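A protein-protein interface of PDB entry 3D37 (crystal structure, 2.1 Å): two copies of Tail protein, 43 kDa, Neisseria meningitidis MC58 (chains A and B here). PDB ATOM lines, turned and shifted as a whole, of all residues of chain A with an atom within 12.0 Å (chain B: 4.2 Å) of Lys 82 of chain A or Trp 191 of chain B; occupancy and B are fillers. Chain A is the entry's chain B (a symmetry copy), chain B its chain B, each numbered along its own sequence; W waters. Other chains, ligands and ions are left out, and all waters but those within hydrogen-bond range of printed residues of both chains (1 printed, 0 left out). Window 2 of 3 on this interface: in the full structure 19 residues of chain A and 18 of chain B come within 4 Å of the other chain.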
ATOM      1  N   ARG A  77      18.892  -8.253 -15.026  1.00  0.00           N
ATOM      2  CA  ARG A  77      18.939  -9.497 -14.277  1.00  0.00           C
ATOM      3  C   ARG A  77      18.088  -9.379 -13.015  1.00  0.00           C
ATOM      4  O   ARG A  77      18.151  -8.405 -12.300  1.00  0.00           O
ATOM      5  CB  ARG A  77      20.387  -9.899 -13.938  1.00  0.00           C
ATOM      6  CG  ARG A  77      20.479 -11.397 -13.608  1.00  0.00           C
ATOM      7  CD  ARG A  77      21.653 -11.781 -12.734  1.00  0.00           C
ATOM      8  NE  ARG A  77      21.342 -11.449 -11.343  1.00  0.00           N
ATOM      9  CZ  ARG A  77      21.593 -12.215 -10.288  1.00  0.00           C
ATOM     10  NH1 ARG A  77      21.272 -11.758  -9.090  1.00  0.00           N
ATOM     11  NH2 ARG A  77      22.160 -13.416 -10.409  1.00  0.00           N
ATOM     12  N   HIS A  78      17.252 -10.379 -12.789  1.00  0.00           N
ATOM     13  CA  HIS A  78      16.577 -10.510 -11.527  1.00  0.00           C
ATOM     14  C   HIS A  78      17.060 -11.774 -10.807  1.00  0.00           C
ATOM     15  O   HIS A  78      16.842 -12.890 -11.295  1.00  0.00           O
ATOM     16  CB  HIS A  78      15.052 -10.536 -11.657  1.00  0.00           C
ATOM     17  CG  HIS A  78      14.390 -10.594 -10.311  1.00  0.00           C
ATOM     18  ND1 HIS A  78      14.632  -9.653  -9.329  1.00  0.00           N
ATOM     19  CD2 HIS A  78      13.604 -11.532  -9.741  1.00  0.00           C
ATOM     20  CE1 HIS A  78      13.998  -9.996  -8.227  1.00  0.00           C
ATOM     21  NE2 HIS A  78      13.355 -11.127  -8.456  1.00  0.00           N
ATOM     22  N   GLY A  79      17.721 -11.583  -9.675  1.00  0.00           N
ATOM     23  CA  GLY A  79      18.216 -12.699  -8.854  1.00  0.00           C
ATOM     24  C   GLY A  79      17.564 -12.775  -7.479  1.00  0.00           C
ATOM     25  O   GLY A  79      17.388 -11.752  -6.826  1.00  0.00           O
ATOM     26  N   LYS A  80      17.227 -13.983  -7.045  1.00  0.00           N
ATOM     27  CA  LYS A  80      16.812 -14.196  -5.671  1.00  0.00           C
ATOM     28  C   LYS A  80      17.132 -15.547  -5.039  1.00  0.00           C
ATOM     29  O   LYS A  80      17.108 -16.599  -5.683  1.00  0.00           O
ATOM     30  CB  LYS A  80      15.310 -13.889  -5.477  1.00  0.00           C
ATOM     31  CG  LYS A  80      14.344 -14.854  -6.060  1.00  0.00           C
ATOM     32  CD  LYS A  80      12.898 -14.383  -5.832  1.00  0.00           C
ATOM     33  CE  LYS A  80      11.953 -15.061  -6.846  1.00  0.00           C
ATOM     34  NZ  LYS A  80      10.531 -14.552  -6.712  1.00  0.00           N
ATOM     35  N   SER A  81      17.419 -15.468  -3.749  1.00  0.00           N
ATOM     36  CA  SER A  81      17.546 -16.610  -2.883  1.00  0.00           C
ATOM     37  C   SER A  81      16.665 -16.372  -1.656  1.00  0.00           C
ATOM     38  O   SER A  81      15.975 -15.342  -1.569  1.00  0.00           O
ATOM     39  CB  SER A  81      18.985 -16.710  -2.461  1.00  0.00           C
ATOM     40  OG  SER A  81      19.287 -15.556  -1.690  1.00  0.00           O
ATOM     41  N   LYS A  82      16.675 -17.329  -0.723  1.00  0.00           N
ATOM     42  CA  LYS A  82      15.888 -17.241   0.504  1.00  0.00           C
ATOM     43  C   LYS A  82      16.131 -15.896   1.220  1.00  0.00           C
ATOM     44  O   LYS A  82      15.206 -15.174   1.475  1.00  0.00           O
ATOM     45  CB  LYS A  82      16.153 -18.460   1.452  1.00  0.00           C
ATOM     46  CG  LYS A  82      17.704 -18.725   1.754  1.00  0.00           C
ATOM     47  CD  LYS A  82      17.976 -19.894   2.761  1.00  0.00           C
ATOM     48  CE  LYS A  82      19.434 -20.435   2.628  1.00  0.00           C
ATOM     49  NZ  LYS A  82      20.515 -19.389   2.506  1.00  0.00           N
ATOM     50  N   GLY A  83      17.357 -15.516   1.480  1.00  0.00           N
ATOM     51  CA  GLY A  83      17.571 -14.226   2.161  1.00  0.00           C
ATOM     52  C   GLY A  83      17.628 -12.918   1.346  1.00  0.00           C
ATOM     53  O   GLY A  83      17.576 -11.834   1.918  1.00  0.00           O
ATOM     54  N   SER A  84      17.714 -12.990   0.024  1.00  0.00           N
ATOM     55  CA  SER A  84      17.908 -11.781  -0.755  1.00  0.00           C
ATOM     56  C   SER A  84      17.307 -11.833  -2.140  1.00  0.00           C
ATOM     57  O   SER A  84      17.091 -12.888  -2.707  1.00  0.00           O
ATOM     58  CB  SER A  84      19.418 -11.457  -0.840  1.00  0.00           C
ATOM     59  OG  SER A  84      20.096 -12.507  -1.517  1.00  0.00           O
ATOM     60  N   ARG A  85      17.098 -10.648  -2.694  1.00  0.00           N
ATOM     61  CA  ARG A  85      16.409 -10.443  -3.956  1.00  0.00           C
ATOM     62  C   ARG A  85      17.133  -9.231  -4.607  1.00  0.00           C
ATOM     63  O   ARG A  85      17.319  -8.199  -3.940  1.00  0.00           O
ATOM     64  CB  ARG A  85      14.925 -10.195  -3.627  1.00  0.00           C
ATOM     65  CG  ARG A  85      13.892 -10.343  -4.742  1.00  0.00           C
ATOM     66  CD  ARG A  85      12.537 -11.128  -4.316  1.00  0.00           C
ATOM     67  NE  ARG A  85      11.925 -10.732  -3.044  1.00  0.00           N
ATOM     68  CZ  ARG A  85      11.373  -9.533  -2.813  1.00  0.00           C
ATOM     69  NH1 ARG A  85      11.367  -8.588  -3.773  1.00  0.00           N
ATOM     70  NH2 ARG A  85      10.844  -9.259  -1.615  1.00  0.00           N
ATOM     71  N   GLU A  86      17.662  -9.352  -5.840  1.00  0.00           N
ATOM     72  CA  GLU A  86      18.143  -8.114  -6.506  1.00  0.00           C
ATOM     73  C   GLU A  86      17.937  -8.037  -8.011  1.00  0.00           C
ATOM     74  O   GLU A  86      17.870  -9.047  -8.713  1.00  0.00           O
ATOM     75  CB  GLU A  86      19.549  -7.632  -6.033  1.00  0.00           C
ATOM     76  CG  GLU A  86      20.774  -8.457  -6.425  1.00  0.00           C
ATOM     77  CD  GLU A  86      22.030  -8.166  -5.572  1.00  0.00           C
ATOM     78  OE1 GLU A  86      21.997  -7.388  -4.562  1.00  0.00           O
ATOM     79  OE2 GLU A  86      23.082  -8.740  -5.919  1.00  0.00           O
ATOM     80  N   CYS B 190       8.127 -24.643  -7.867  1.00  0.00           N
ATOM     81  CA  CYS B 190       7.603 -23.391  -7.374  1.00  0.00           C
ATOM     82  C   CYS B 190       8.549 -22.702  -6.412  1.00  0.00           C
ATOM     83  O   CYS B 190       9.403 -23.314  -5.790  1.00  0.00           O
ATOM     84  CB  CYS B 190       6.194 -23.565  -6.752  1.00  0.00           C
ATOM     85  SG  CYS B 190       6.136 -24.700  -5.294  1.00  0.00           S
ATOM     86  N   TRP B 191       8.389 -21.395  -6.367  1.00  0.00           N
ATOM     87  CA  TRP B 191       9.029 -20.515  -5.421  1.00  0.00           C
ATOM     88  C   TRP B 191       8.017 -20.069  -4.358  1.00  0.00           C
ATOM     89  O   TRP B 191       6.893 -19.693  -4.681  1.00  0.00           O
ATOM     90  CB  TRP B 191       9.498 -19.248  -6.142  1.00  0.00           C
ATOM     91  CG  TRP B 191      10.052 -18.216  -5.218  1.00  0.00           C
ATOM     92  CD1 TRP B 191       9.421 -17.071  -4.791  1.00  0.00           C
ATOM     93  CD2 TRP B 191      11.343 -18.196  -4.627  1.00  0.00           C
ATOM     94  NE1 TRP B 191      10.249 -16.350  -3.976  1.00  0.00           N
ATOM     95  CE2 TRP B 191      11.430 -17.019  -3.847  1.00  0.00           C
ATOM     96  CE3 TRP B 191      12.448 -19.045  -4.684  1.00  0.00           C
ATOM     97  CZ2 TRP B 191      12.559 -16.683  -3.153  1.00  0.00           C
ATOM     98  CZ3 TRP B 191      13.556 -18.722  -3.958  1.00  0.00           C
ATOM     99  CH2 TRP B 191      13.608 -17.557  -3.200  1.00  0.00           C
ATOM    100  N   SER B 192       8.449 -20.050  -3.104  1.00  0.00           N
ATOM    101  CA  SER B 192       7.609 -19.546  -2.021  1.00  0.00           C
ATOM    102  C   SER B 192       8.553 -19.359  -0.877  1.00  0.00           C
ATOM    103  O   SER B 192       9.333 -20.275  -0.566  1.00  0.00           O
ATOM    104  CB  SER B 192       6.447 -20.545  -1.696  1.00  0.00           C
ATOM    105  OG  SER B 192       5.401 -19.988  -0.868  1.00  0.00           O
ATOM    106  N   ARG B 193       8.496 -18.181  -0.284  1.00  0.00           N
ATOM    107  CA  ARG B 193       9.089 -17.895   1.009  1.00  0.00           C
ATOM    108  C   ARG B 193       8.205 -18.419   2.173  1.00  0.00           C
ATOM    109  O   ARG B 193       8.683 -18.626   3.281  1.00  0.00           O
ATOM    110  CB  ARG B 193       9.452 -16.417   1.155  1.00  0.00           C
ATOM    111  CG  ARG B 193      10.390 -15.896   0.080  1.00  0.00           C
ATOM    112  CD  ARG B 193      10.723 -14.440   0.202  1.00  0.00           C
ATOM    113  NE  ARG B 193       9.617 -13.589  -0.172  1.00  0.00           N
ATOM    114  CZ  ARG B 193       9.245 -12.466   0.453  1.00  0.00           C
ATOM    115  NH1 ARG B 193       8.205 -11.792   0.003  1.00  0.00           N
ATOM    116  NH2 ARG B 193       9.883 -11.999   1.511  1.00  0.00           N
ATOM    117  N   CYS B 198       7.734 -26.043  -1.698  1.00  0.00           N
ATOM    118  CA  CYS B 198       8.457 -25.422  -2.820  1.00  0.00           C
ATOM    119  C   CYS B 198       9.968 -25.662  -2.773  1.00  0.00           C
ATOM    120  O   CYS B 198      10.645 -25.459  -1.770  1.00  0.00           O
ATOM    121  CB  CYS B 198       8.134 -23.931  -2.909  1.00  0.00           C
ATOM    122  SG  CYS B 198       6.515 -23.519  -3.627  1.00  0.00           S
ATOM    123  N   ILE B 200      12.535 -24.602  -5.102  1.00  0.00           N
ATOM    124  CA  ILE B 200      13.492 -23.710  -5.700  1.00  0.00           C
ATOM    125  C   ILE B 200      14.268 -22.981  -4.599  1.00  0.00           C
ATOM    126  O   ILE B 200      13.665 -22.248  -3.817  1.00  0.00           O
ATOM    127  CB  ILE B 200      12.764 -22.666  -6.642  1.00  0.00           C
ATOM    128  CG1 ILE B 200      12.073 -23.368  -7.821  1.00  0.00           C
ATOM    129  CG2 ILE B 200      13.735 -21.598  -7.090  1.00  0.00           C
ATOM    130  CD1 ILE B 200      11.153 -22.521  -8.602  1.00  0.00           C
ATOM    131  N   GLU B 201      15.600 -23.152  -4.592  1.00  0.00           N
ATOM    132  CA  GLU B 201      16.501 -22.524  -3.650  1.00  0.00           C
ATOM    133  C   GLU B 201      17.028 -21.202  -4.173  1.00  0.00           C
ATOM    134  O   GLU B 201      17.185 -20.231  -3.439  1.00  0.00           O
ATOM    135  CB  GLU B 201      17.650 -23.473  -3.307  1.00  0.00           C
ATOM    136  CG  GLU B 201      17.112 -24.832  -2.844  1.00  0.00           C
ATOM    137  CD  GLU B 201      18.173 -25.780  -2.292  1.00  0.00           C
ATOM    138  OE1 GLU B 201      19.414 -25.622  -2.573  1.00  0.00           O
ATOM    139  OE2 GLU B 201      17.732 -26.679  -1.530  1.00  0.00           O
ATOM    140  N   ILE B 304       6.244 -22.069 -11.397  1.00  0.00           N
ATOM    141  CA  ILE B 304       5.300 -21.157 -10.740  1.00  0.00           C
ATOM    142  C   ILE B 304       6.027 -20.327  -9.718  1.00  0.00           C
ATOM    143  O   ILE B 304       6.648 -20.846  -8.793  1.00  0.00           O
ATOM    144  CB  ILE B 304       4.112 -21.860 -10.009  1.00  0.00           C
ATOM    145  CG1 ILE B 304       3.450 -22.930 -10.893  1.00  0.00           C
ATOM    146  CG2 ILE B 304       3.074 -20.769  -9.543  1.00  0.00           C
ATOM    147  CD1 ILE B 304       2.511 -23.897 -10.107  1.00  0.00           C
ATOM    148  N   ASP B 305       5.966 -19.028  -9.907  1.00  0.00           N
ATOM    149  CA  ASP B 305       6.525 -18.121  -8.949  1.00  0.00           C
ATOM    150  C   ASP B 305       5.433 -17.092  -8.750  1.00  0.00           C
ATOM    151  O   ASP B 305       5.399 -16.069  -9.448  1.00  0.00           O
ATOM    152  CB  ASP B 305       7.815 -17.498  -9.495  1.00  0.00           C
ATOM    153  CG  ASP B 305       8.479 -16.543  -8.515  1.00  0.00           C
ATOM    154  OD1 ASP B 305       7.806 -16.028  -7.567  1.00  0.00           O
ATOM    155  OD2 ASP B 305       9.691 -16.309  -8.689  1.00  0.00           O
ATOM    156  N   GLU B 307       5.008 -15.023  -6.639  1.00  0.00           N
ATOM    157  CA  GLU B 307       5.594 -13.740  -6.231  1.00  0.00           C
ATOM    158  C   GLU B 307       6.092 -12.860  -7.405  1.00  0.00           C
ATOM    159  O   GLU B 307       5.916 -11.644  -7.375  1.00  0.00           O
ATOM    160  CB  GLU B 307       6.696 -13.995  -5.174  1.00  0.00           C
ATOM    161  CG  GLU B 307       7.641 -12.837  -4.838  1.00  0.00           C
ATOM    162  CD  GLU B 307       8.681 -13.233  -3.767  1.00  0.00           C
ATOM    163  OE1 GLU B 307       8.310 -13.924  -2.785  1.00  0.00           O
ATOM    164  OE2 GLU B 307       9.878 -12.878  -3.913  1.00  0.00           O
HETATM  165  O   HOH W   1      17.932 -19.779  -1.036  1.00  0.00           O
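Of the 10 printed residues of chain B, 5 touch a printed residue of chain A. Printed residues of chain B that touch a printed residue of chain A: Trp 191, Arg 193, Glu 201, Asp 305 and Glu 307. Along chain B the printed residues that touch a printed residue of chain A span positions 191 to 307. Among the printed residues, 8 pairs touch across the chains. Among the printed residues, Asp or Glu carboxylates within 4 Å of a Lys or Arg side-chain nitrogen of the other chain: Lys 80 of chain A with Asp 305 of chain B, Lys 80 of chain A with Glu 307 of chain B and Arg 85 of chain A with Glu 307 of chain B.
Printed residues of chain B within 4 Å of Lys 80 of chain A: Trp 191 (3.3 Å), Asp 305 (2.8 Å) and Glu 307 (3.3 Å). Printed residues of chain B within 4 Å of Ser 81 of chain A: Trp 191 (3.6 Å) and Glu 201 (3.7 Å). Gly 83 of chain A touches none of the printed residues of chain B. Of the printed residues of chain B, Arg 85 of chain A touches Arg 193 and Glu 307. No residue of chain A comes within 4 Å of Cys 190 of chain B. Trp 191 of chain B touches just these residues of chain A: Lys 80, Ser 81 and Lys 82. No residue of chain A comes within 4 Å of Ser 192 of chain B. Of the printed residues of chain A, Glu 201 of chain B touches Ser 81. No residue of chain A comes within 4 Å of Ile 304 of chain B. The nearest printed residue of chain A that does not touch Glu 201 of chain B is Lys 82 of chain A (4.01 Å).
Water W1 bridges O of Glu 201 of chain B (2.6 Å) and N of Lys 82 of chain A (2.8 Å).
No position is printed for both chains. Of the 8 pairs that touch across the chains among the printed residues, none has its exchanged pair printed and touching as well.
N of Trp 191 of chain B sits at hydrogen-bond distance from O of Ile 304 of chain B. The indole nitrogen (NE1) of Trp 191 of chain B is in hydrogen-bond range of the side-chain carboxylate (OE1) of Glu 307 of chain B, at 3.3 Å. The side-chain carboxylate of Glu 307 of chain B lies within salt-bridge range of the guanidinium group of Arg 193 of chain B, at 2.9 Å. OD1 of Asp 305 of chain B lies close to N of Glu 307 of chain B (3.1 Å). The side-chain hydroxyl (OG) of Ser 84 of chain A lies within hydrogen-bond range of the side-chain hydroxyl (OG) of Ser 81 of chain A (3.2 Å). The side-chain sulfur (SG) of Cys 190 of chain B is disulfide-bonded to the side-chain sulfur (SG) of Cys 198 of chain B (2.1 Å).
NZ of Lys 80 of chain A lies within salt-bridge range of OD2 of Asp 305 of chain B, 2.8 Å away. The side-chain amino group (NZ) of Lys 80 of chain A lies within salt-bridge range of the side-chain carboxylate (OE2) of Glu 307 of chain B (3.3 Å). The side-chain carboxylate (OE2) of Glu 307 of chain B lies within salt-bridge range of the guanidinium group (NE) of Arg 85 of chain A. The side-chain amino group of Lys 80 of chain A lies close to the indole nitrogen of Trp 191 of chain B (3.3 Å).
Trp 191 of chain B touches Ser 81 of chain A. CA of Ser 81 of chain A touches O of Glu 201 of chain B (3.7 Å). Lys 82 of chain A touches Trp 191 of chain B. Arg 85 of chain A touches Arg 193 of chain B.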
